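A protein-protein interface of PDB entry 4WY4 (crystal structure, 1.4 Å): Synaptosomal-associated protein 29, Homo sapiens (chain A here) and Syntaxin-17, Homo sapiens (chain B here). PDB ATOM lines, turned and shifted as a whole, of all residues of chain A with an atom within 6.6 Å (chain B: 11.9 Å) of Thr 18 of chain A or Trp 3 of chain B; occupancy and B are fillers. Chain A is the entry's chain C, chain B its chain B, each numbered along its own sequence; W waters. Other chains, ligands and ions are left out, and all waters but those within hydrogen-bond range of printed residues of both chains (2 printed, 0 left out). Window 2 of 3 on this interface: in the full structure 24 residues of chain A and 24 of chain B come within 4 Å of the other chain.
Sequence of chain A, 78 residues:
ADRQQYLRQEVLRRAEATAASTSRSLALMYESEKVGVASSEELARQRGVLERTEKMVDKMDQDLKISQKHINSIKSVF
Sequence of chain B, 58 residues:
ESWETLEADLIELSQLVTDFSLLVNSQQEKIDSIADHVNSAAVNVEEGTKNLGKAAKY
OE2 of Glu 7 of chain B lies within hydrogen-bond range of OG of Ser 21 of chain A.
The side-chain carboxylate (OE1) of Glu 1 of chain B lies within hydrogen-bond range of the indole nitrogen (NE1) of Trp 3 of chain B, 2.9 Å away.
The backbone carbonyl oxygen of Arg 14 of chain A sits at hydrogen-bond distance from the side-chain hydroxyl of Thr 18 of chain A (2.8 Å).
The backbone carbonyl oxygen of Thr 18 of chain A lies within hydrogen-bond range of the side-chain hydroxyl of Thr 22 of chain A (2.9 Å).
The side-chain hydroxyl of Thr 22 of chain A sits at hydrogen-bond distance from the backbone carbonyl oxygen of Ala 19 of chain A (3.3 Å).
The backbone carbonyl oxygen (O) of Ser 21 of chain A is in hydrogen-bond range of the side-chain hydroxyl (OG) of Ser 25 of chain A (3.4 Å).
CG2 of Thr 18 of chain A touches CD1 of Trp 3 of chain B, at 3.4 Å.
O of Trp 3 of chain B touches OG of Ser 21 of chain A, at 3.8 Å.
Ser 21 of chain A touches Glu 4 of chain B (OG to CA, 3.5 Å).
Trp 3 of chain B touches Thr 22 of chain A (CB to CG2, 3.9 Å).
Glu 7 of chain B touches Ser 25 of chain A (CG to OG, 3.3 Å).
CD1 of Leu 10 of chain B touches CB of Ser 25 of chain A (3.4 Å).
No residue of chain B comes within 4 Å of Arg 14 of chain A.
No residue of chain B comes within 4 Å of Ala 15 of chain A.
No residue of chain B comes within 4 Å of Glu 16 of chain A.
Of the printed residues of chain B, Thr 18 of chain A touches Trp 3 (3.4 Å).
No residue of chain B comes within 4 Å of Ala 20 of chain A.
Of the printed residues of chain B, Ser 21 of chain A touches Trp 3 (3.8 Å), Glu 4 (3.5 Å) and Glu 7 (2.5 Å).
Of the printed residues of chain B, Thr 22 of chain A touches Trp 3 (3.9 Å).
Printed residues of chain B within 4 Å of Ser 25 of chain A: Glu 7 (3.3 Å) and Leu 10 (3.4 Å).
Trp 3 of chain B touches just these residues of chain A: Thr 18 (3.4 Å), Ser 21 (3.8 Å) and Thr 22 (3.9 Å).
Printed residues of chain A within 4 Å of Glu 4 of chain B: Ser 21.
Printed residues of chain A within 4 Å of Glu 7 of chain B: Ser 21 (2.5 Å) and Ser 25 (3.3 Å).
Printed residues of chain A within 4 Å of Leu 10 of chain B: Ser 25.
The nearest residue of chain B that does not touch Thr 18 of chain A is Glu 1 of chain B (4.3 Å).
The nearest printed residue of chain A that does not touch Glu 4 of chain B is Ala 17 of chain A (5.9 Å).
Of the 11 printed residues of chain B, 4 touch a printed residue of chain A.
Along chain B the printed residues that touch a printed residue of chain A span positions 3 to 10.
Among the printed residues, no Asp or Glu carboxylate lies within 4 Å of a Lys or Arg side-chain nitrogen of the other chain.
Water W2 lies within hydrogen-bond range of the backbone carbonyl oxygen of Trp 3 of chain B (2.8 Å), the side-chain hydroxyl of Ser 25 of chain A (2.8 Å) and the side-chain hydroxyl of Ser 21 of chain A (2.9 Å).
Water W1 lies within hydrogen-bond range of OG1 of Thr 18 of chain A and O of Glu 1 of chain B.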
ATOM      1  N   ARG A  13     -17.811  -2.096 -13.630  1.00  0.00           N
ATOM      2  CA  ARG A  13     -17.519  -2.511 -14.988  1.00  0.00           C
ATOM      3  C   ARG A  13     -18.217  -3.833 -15.270  1.00  0.00           C
ATOM      4  O   ARG A  13     -18.845  -4.024 -16.339  1.00  0.00           O
ATOM      5  CB  ARG A  13     -15.997  -2.637 -15.207  1.00  0.00           C
ATOM      6  CG  ARG A  13     -15.652  -3.035 -16.639  1.00  0.00           C
ATOM      7  CD  ARG A  13     -14.170  -3.226 -16.841  1.00  0.00           C
ATOM      8  NE  ARG A  13     -13.655  -4.318 -16.025  1.00  0.00           N
ATOM      9  CZ  ARG A  13     -12.361  -4.559 -15.816  1.00  0.00           C
ATOM     10  NH1 ARG A  13     -12.013  -5.586 -15.053  1.00  0.00           N
ATOM     11  NH2 ARG A  13     -11.417  -3.774 -16.334  1.00  0.00           N
ATOM     12  N   ARG A  14     -18.140  -4.747 -14.308  1.00  0.00           N
ATOM     13  CA  ARG A  14     -18.744  -6.069 -14.482  1.00  0.00           C
ATOM     14  C   ARG A  14     -20.274  -5.981 -14.532  1.00  0.00           C
ATOM     15  O   ARG A  14     -20.923  -6.665 -15.331  1.00  0.00           O
ATOM     16  CB  ARG A  14     -18.302  -7.009 -13.359  1.00  0.00           C
ATOM     17  CG  ARG A  14     -18.573  -8.476 -13.680  1.00  0.00           C
ATOM     18  CD  ARG A  14     -17.991  -9.418 -12.633  1.00  0.00           C
ATOM     19  NE  ARG A  14     -18.877  -9.545 -11.483  1.00  0.00           N
ATOM     20  CZ  ARG A  14     -18.608  -9.094 -10.260  1.00  0.00           C
ATOM     21  NH1 ARG A  14     -17.462  -8.475 -10.001  1.00  0.00           N
ATOM     22  NH2 ARG A  14     -19.498  -9.263  -9.288  1.00  0.00           N
ATOM     23  N   ALA A  15     -20.861  -5.117 -13.721  1.00  0.00           N
ATOM     24  CA  ALA A  15     -22.322  -4.967 -13.687  1.00  0.00           C
ATOM     25  C   ALA A  15     -22.812  -4.380 -15.007  1.00  0.00           C
ATOM     26  O   ALA A  15     -23.807  -4.845 -15.582  1.00  0.00           O
ATOM     27  CB  ALA A  15     -22.737  -4.087 -12.493  1.00  0.00           C
ATOM     28  N   GLU A  16     -22.108  -3.385 -15.523  1.00  0.00           N
ATOM     29  CA  GLU A  16     -22.456  -2.777 -16.788  1.00  0.00           C
ATOM     30  C   GLU A  16     -22.358  -3.832 -17.882  1.00  0.00           C
ATOM     31  O   GLU A  16     -23.237  -3.927 -18.740  1.00  0.00           O
ATOM     32  CB  GLU A  16     -21.542  -1.579 -17.117  1.00  0.00           C
ATOM     33  CG  GLU A  16     -22.027  -0.756 -18.344  1.00  0.00           C
ATOM     34  CD  GLU A  16     -21.757  -1.425 -19.699  1.00  0.00           C
ATOM     35  OE1 GLU A  16     -20.776  -2.191 -19.817  1.00  0.00           O
ATOM     36  OE2 GLU A  16     -22.524  -1.187 -20.661  1.00  0.00           O
ATOM     37  N   ALA A  17     -21.281  -4.609 -17.879  1.00  0.00           N
ATOM     38  CA  ALA A  17     -21.056  -5.597 -18.925  1.00  0.00           C
ATOM     39  C   ALA A  17     -22.099  -6.709 -18.866  1.00  0.00           C
ATOM     40  O   ALA A  17     -22.575  -7.185 -19.909  1.00  0.00           O
ATOM     41  CB  ALA A  17     -19.633  -6.183 -18.809  1.00  0.00           C
ATOM     42  N   THR A  18     -22.479  -7.102 -17.660  1.00  0.00           N
ATOM     43  CA  THR A  18     -23.466  -8.164 -17.473  1.00  0.00           C
ATOM     44  C   THR A  18     -24.872  -7.683 -17.874  1.00  0.00           C
ATOM     45  O   THR A  18     -25.623  -8.413 -18.511  1.00  0.00           O
ATOM     46  CB  THR A  18     -23.442  -8.658 -16.021  1.00  0.00           C
ATOM     47  OG1 THR A  18     -22.141  -9.198 -15.747  1.00  0.00           O
ATOM     48  CG2 THR A  18     -24.467  -9.747 -15.785  1.00  0.00           C
ATOM     49  N   ALA A  19     -25.203  -6.448 -17.530  1.00  0.00           N
ATOM     50  CA  ALA A  19     -26.469  -5.844 -17.934  1.00  0.00           C
ATOM     51  C   ALA A  19     -26.539  -5.803 -19.455  1.00  0.00           C
ATOM     52  O   ALA A  19     -27.534  -6.232 -20.051  1.00  0.00           O
ATOM     53  CB  ALA A  19     -26.618  -4.454 -17.352  1.00  0.00           C
ATOM     54  N   ALA A  20     -25.478  -5.336 -20.096  1.00  0.00           N
ATOM     55  CA  ALA A  20     -25.450  -5.234 -21.550  1.00  0.00           C
ATOM     56  C   ALA A  20     -25.557  -6.602 -22.199  1.00  0.00           C
ATOM     57  O   ALA A  20     -26.294  -6.793 -23.174  1.00  0.00           O
ATOM     58  CB  ALA A  20     -24.156  -4.526 -22.012  1.00  0.00           C
ATOM     59  N   SER A  21     -24.759  -7.548 -21.717  1.00  0.00           N
ATOM     60  CA  SER A  21     -24.753  -8.891 -22.283  1.00  0.00           C
ATOM     61  C   SER A  21     -26.099  -9.593 -22.127  1.00  0.00           C
ATOM     62  O   SER A  21     -26.643 -10.179 -23.102  1.00  0.00           O
ATOM     63  CB  SER A  21     -23.650  -9.731 -21.624  1.00  0.00           C
ATOM     64  OG  SER A  21     -23.730 -11.067 -22.078  1.00  0.00           O
ATOM     65  N   THR A  22     -26.670  -9.534 -20.927  1.00  0.00           N
ATOM     66  CA  THR A  22     -27.956 -10.203 -20.729  1.00  0.00           C
ATOM     67  C   THR A  22     -29.076  -9.500 -21.517  1.00  0.00           C
ATOM     68  O   THR A  22     -30.044 -10.158 -21.909  1.00  0.00           O
ATOM     69  CB  THR A  22     -28.362 -10.335 -19.236  1.00  0.00           C
ATOM     70  OG1 THR A  22     -28.407  -9.048 -18.598  1.00  0.00           O
ATOM     71  CG2 THR A  22     -27.390 -11.248 -18.494  1.00  0.00           C
ATOM     72  N   SER A  23     -28.947  -8.200 -21.774  1.00  0.00           N
ATOM     73  CA  SER A  23     -29.909  -7.500 -22.622  1.00  0.00           C
ATOM     74  C   SER A  23     -29.783  -7.970 -24.071  1.00  0.00           C
ATOM     75  O   SER A  23     -30.801  -8.107 -24.770  1.00  0.00           O
ATOM     76  CB  SER A  23     -29.735  -5.987 -22.553  1.00  0.00           C
ATOM     77  OG  SER A  23     -30.272  -5.501 -21.337  1.00  0.00           O
ATOM     78  N   SER A  25     -28.714 -10.956 -24.980  1.00  0.00           N
ATOM     79  CA  SER A  25     -29.279 -12.313 -24.943  1.00  0.00           C
ATOM     80  C   SER A  25     -30.804 -12.297 -24.967  1.00  0.00           C
ATOM     81  O   SER A  25     -31.426 -13.062 -25.707  1.00  0.00           O
ATOM     82  CB  SER A  25     -28.765 -13.054 -23.695  1.00  0.00           C
ATOM     83  OG  SER A  25     -27.422 -13.444 -23.899  1.00  0.00           O
ATOM     84  N   GLU B   1     -20.230 -13.479 -11.979  1.00  0.00           N
ATOM     85  CA  GLU B   1     -20.774 -14.356 -13.015  1.00  0.00           C
ATOM     86  C   GLU B   1     -20.298 -13.956 -14.410  1.00  0.00           C
ATOM     87  O   GLU B   1     -20.066 -12.777 -14.690  1.00  0.00           O
ATOM     88  CB  GLU B   1     -22.302 -14.354 -12.983  1.00  0.00           C
ATOM     89  CG  GLU B   1     -22.915 -15.321 -11.986  1.00  0.00           C
ATOM     90  CD  GLU B   1     -24.076 -14.706 -11.235  1.00  0.00           C
ATOM     91  OE1 GLU B   1     -24.664 -13.728 -11.745  1.00  0.00           O
ATOM     92  OE2 GLU B   1     -24.390 -15.193 -10.131  1.00  0.00           O
ATOM     93  N   SER B   2     -20.161 -14.954 -15.280  1.00  0.00           N
ATOM     94  CA  SER B   2     -19.766 -14.727 -16.665  1.00  0.00           C
ATOM     95  C   SER B   2     -20.926 -15.059 -17.591  1.00  0.00           C
ATOM     96  O   SER B   2     -21.077 -16.203 -18.011  1.00  0.00           O
ATOM     97  CB  SER B   2     -18.545 -15.570 -17.026  1.00  0.00           C
ATOM     98  N   TRP B   3     -21.743 -14.059 -17.902  1.00  0.00           N
ATOM     99  CA  TRP B   3     -22.965 -14.291 -18.674  1.00  0.00           C
ATOM    100  C   TRP B   3     -22.766 -14.230 -20.192  1.00  0.00           C
ATOM    101  O   TRP B   3     -23.647 -14.648 -20.948  1.00  0.00           O
ATOM    102  CB  TRP B   3     -24.047 -13.290 -18.230  1.00  0.00           C
ATOM    103  CG  TRP B   3     -24.623 -13.650 -16.886  1.00  0.00           C
ATOM    104  CD1 TRP B   3     -24.292 -13.108 -15.665  1.00  0.00           C
ATOM    105  CD2 TRP B   3     -25.591 -14.673 -16.618  1.00  0.00           C
ATOM    106  NE1 TRP B   3     -25.022 -13.715 -14.667  1.00  0.00           N
ATOM    107  CE2 TRP B   3     -25.817 -14.685 -15.222  1.00  0.00           C
ATOM    108  CE3 TRP B   3     -26.287 -15.582 -17.423  1.00  0.00           C
ATOM    109  CZ2 TRP B   3     -26.712 -15.568 -14.618  1.00  0.00           C
ATOM    110  CZ3 TRP B   3     -27.175 -16.459 -16.821  1.00  0.00           C
ATOM    111  CH2 TRP B   3     -27.384 -16.442 -15.433  1.00  0.00           C
ATOM    112  N   GLU B   4     -21.620 -13.722 -20.640  1.00  0.00           N
ATOM    113  CA  GLU B   4     -21.341 -13.586 -22.076  1.00  0.00           C
ATOM    114  C   GLU B   4     -21.320 -14.933 -22.783  1.00  0.00           C
ATOM    115  O   GLU B   4     -21.543 -15.007 -23.997  1.00  0.00           O
ATOM    116  CB  GLU B   4     -20.004 -12.863 -22.320  1.00  0.00           C
ATOM    117  CG  GLU B   4     -20.144 -11.528 -23.049  1.00  0.00           C
ATOM    118  CD  GLU B   4     -18.872 -11.096 -23.760  1.00  0.00           C
ATOM    119  OE1 GLU B   4     -17.833 -10.917 -23.088  1.00  0.00           O
ATOM    120  OE2 GLU B   4     -18.916 -10.933 -24.999  1.00  0.00           O
ATOM    121  N   THR B   5     -21.061 -16.000 -22.034  1.00  0.00           N
ATOM    122  CA  THR B   5     -21.082 -17.332 -22.622  1.00  0.00           C
ATOM    123  C   THR B   5     -22.496 -17.683 -23.087  1.00  0.00           C
ATOM    124  O   THR B   5     -22.685 -18.407 -24.076  1.00  0.00           O
ATOM    125  CB  THR B   5     -20.554 -18.411 -21.632  1.00  0.00           C
ATOM    126  OG1 THR B   5     -20.763 -19.716 -22.186  1.00  0.00           O
ATOM    127  CG2 THR B   5     -21.254 -18.324 -20.301  1.00  0.00           C
ATOM    128  N   LEU B   6     -23.498 -17.151 -22.399  1.00  0.00           N
ATOM    129  CA  LEU B   6     -24.887 -17.411 -22.795  1.00  0.00           C
ATOM    130  C   LEU B   6     -25.219 -16.798 -24.164  1.00  0.00           C
ATOM    131  O   LEU B   6     -25.992 -17.381 -24.946  1.00  0.00           O
ATOM    132  CB  LEU B   6     -25.839 -16.879 -21.728  1.00  0.00           C
ATOM    133  CG  LEU B   6     -27.331 -17.132 -21.888  1.00  0.00           C
ATOM    134  CD1 LEU B   6     -27.603 -18.613 -21.735  1.00  0.00           C
ATOM    135  CD2 LEU B   6     -28.109 -16.335 -20.845  1.00  0.00           C
ATOM    136  N   GLU B   7     -24.651 -15.640 -24.481  1.00  0.00           N
ATOM    137  CA  GLU B   7     -24.869 -14.994 -25.786  1.00  0.00           C
ATOM    138  C   GLU B   7     -24.546 -15.897 -26.970  1.00  0.00           C
ATOM    139  O   GLU B   7     -25.329 -15.995 -27.914  1.00  0.00           O
ATOM    140  CB  GLU B   7     -24.029 -13.733 -25.934  1.00  0.00           C
ATOM    141  CG  GLU B   7     -24.426 -12.588 -25.075  1.00  0.00           C
ATOM    142  CD  GLU B   7     -23.588 -11.356 -25.377  1.00  0.00           C
ATOM    143  OE1 GLU B   7     -23.592 -10.912 -26.545  1.00  0.00           O
ATOM    144  OE2 GLU B   7     -22.898 -10.858 -24.465  1.00  0.00           O
ATOM    145  N   ALA B   8     -23.372 -16.521 -26.944  1.00  0.00           N
ATOM    146  CA  ALA B   8     -22.970 -17.420 -28.020  1.00  0.00           C
ATOM    147  C   ALA B   8     -23.974 -18.558 -28.215  1.00  0.00           C
ATOM    148  O   ALA B   8     -24.299 -18.920 -29.351  1.00  0.00           O
ATOM    149  CB  ALA B   8     -21.580 -17.984 -27.747  1.00  0.00           C
ATOM    150  N   ASP B   9     -24.469 -19.119 -27.111  1.00  0.00           N
ATOM    151  CA  ASP B   9     -25.437 -20.209 -27.167  1.00  0.00           C
ATOM    152  C   ASP B   9     -26.743 -19.742 -27.810  1.00  0.00           C
ATOM    153  O   ASP B   9     -27.396 -20.477 -28.573  1.00  0.00           O
ATOM    154  CB  ASP B   9     -25.721 -20.765 -25.772  1.00  0.00           C
ATOM    155  CG  ASP B   9     -24.524 -21.465 -25.155  1.00  0.00           C
ATOM    156  OD1 ASP B   9     -23.551 -21.767 -25.873  1.00  0.00           O
ATOM    157  OD2 ASP B   9     -24.586 -21.743 -23.943  1.00  0.00           O
ATOM    158  N   LEU B  10     -27.136 -18.516 -27.517  1.00  0.00           N
ATOM    159  CA  LEU B  10     -28.392 -17.982 -28.027  1.00  0.00           C
ATOM    160  C   LEU B  10     -28.266 -17.578 -29.476  1.00  0.00           C
ATOM    161  O   LEU B  10     -29.245 -17.668 -30.223  1.00  0.00           O
ATOM    162  CB  LEU B  10     -28.857 -16.803 -27.181  1.00  0.00           C
ATOM    163  CG  LEU B  10     -29.471 -17.273 -25.853  1.00  0.00           C
ATOM    164  CD1 LEU B  10     -29.618 -16.144 -24.868  1.00  0.00           C
ATOM    165  CD2 LEU B  10     -30.830 -17.954 -26.087  1.00  0.00           C
ATOM    166  N   ILE B  11     -27.063 -17.191 -29.897  1.00  0.00           N
ATOM    167  CA  ILE B  11     -26.799 -16.941 -31.311  1.00  0.00           C
ATOM    168  C   ILE B  11     -26.949 -18.237 -32.094  1.00  0.00           C
ATOM    169  O   ILE B  11     -27.576 -18.265 -33.149  1.00  0.00           O
ATOM    170  CB  ILE B  11     -25.387 -16.354 -31.520  1.00  0.00           C
ATOM    171  CG1 ILE B  11     -25.340 -14.927 -30.994  1.00  0.00           C
ATOM    172  CG2 ILE B  11     -24.998 -16.388 -32.982  1.00  0.00           C
ATOM    173  CD1 ILE B  11     -23.925 -14.397 -30.829  1.00  0.00           C
HETATM  174  O   HOH W   1     -21.750 -10.697 -13.338  1.00  0.00           O
HETATM  175  O   HOH W   2     -25.822 -13.015 -21.595  1.00  0.00           O
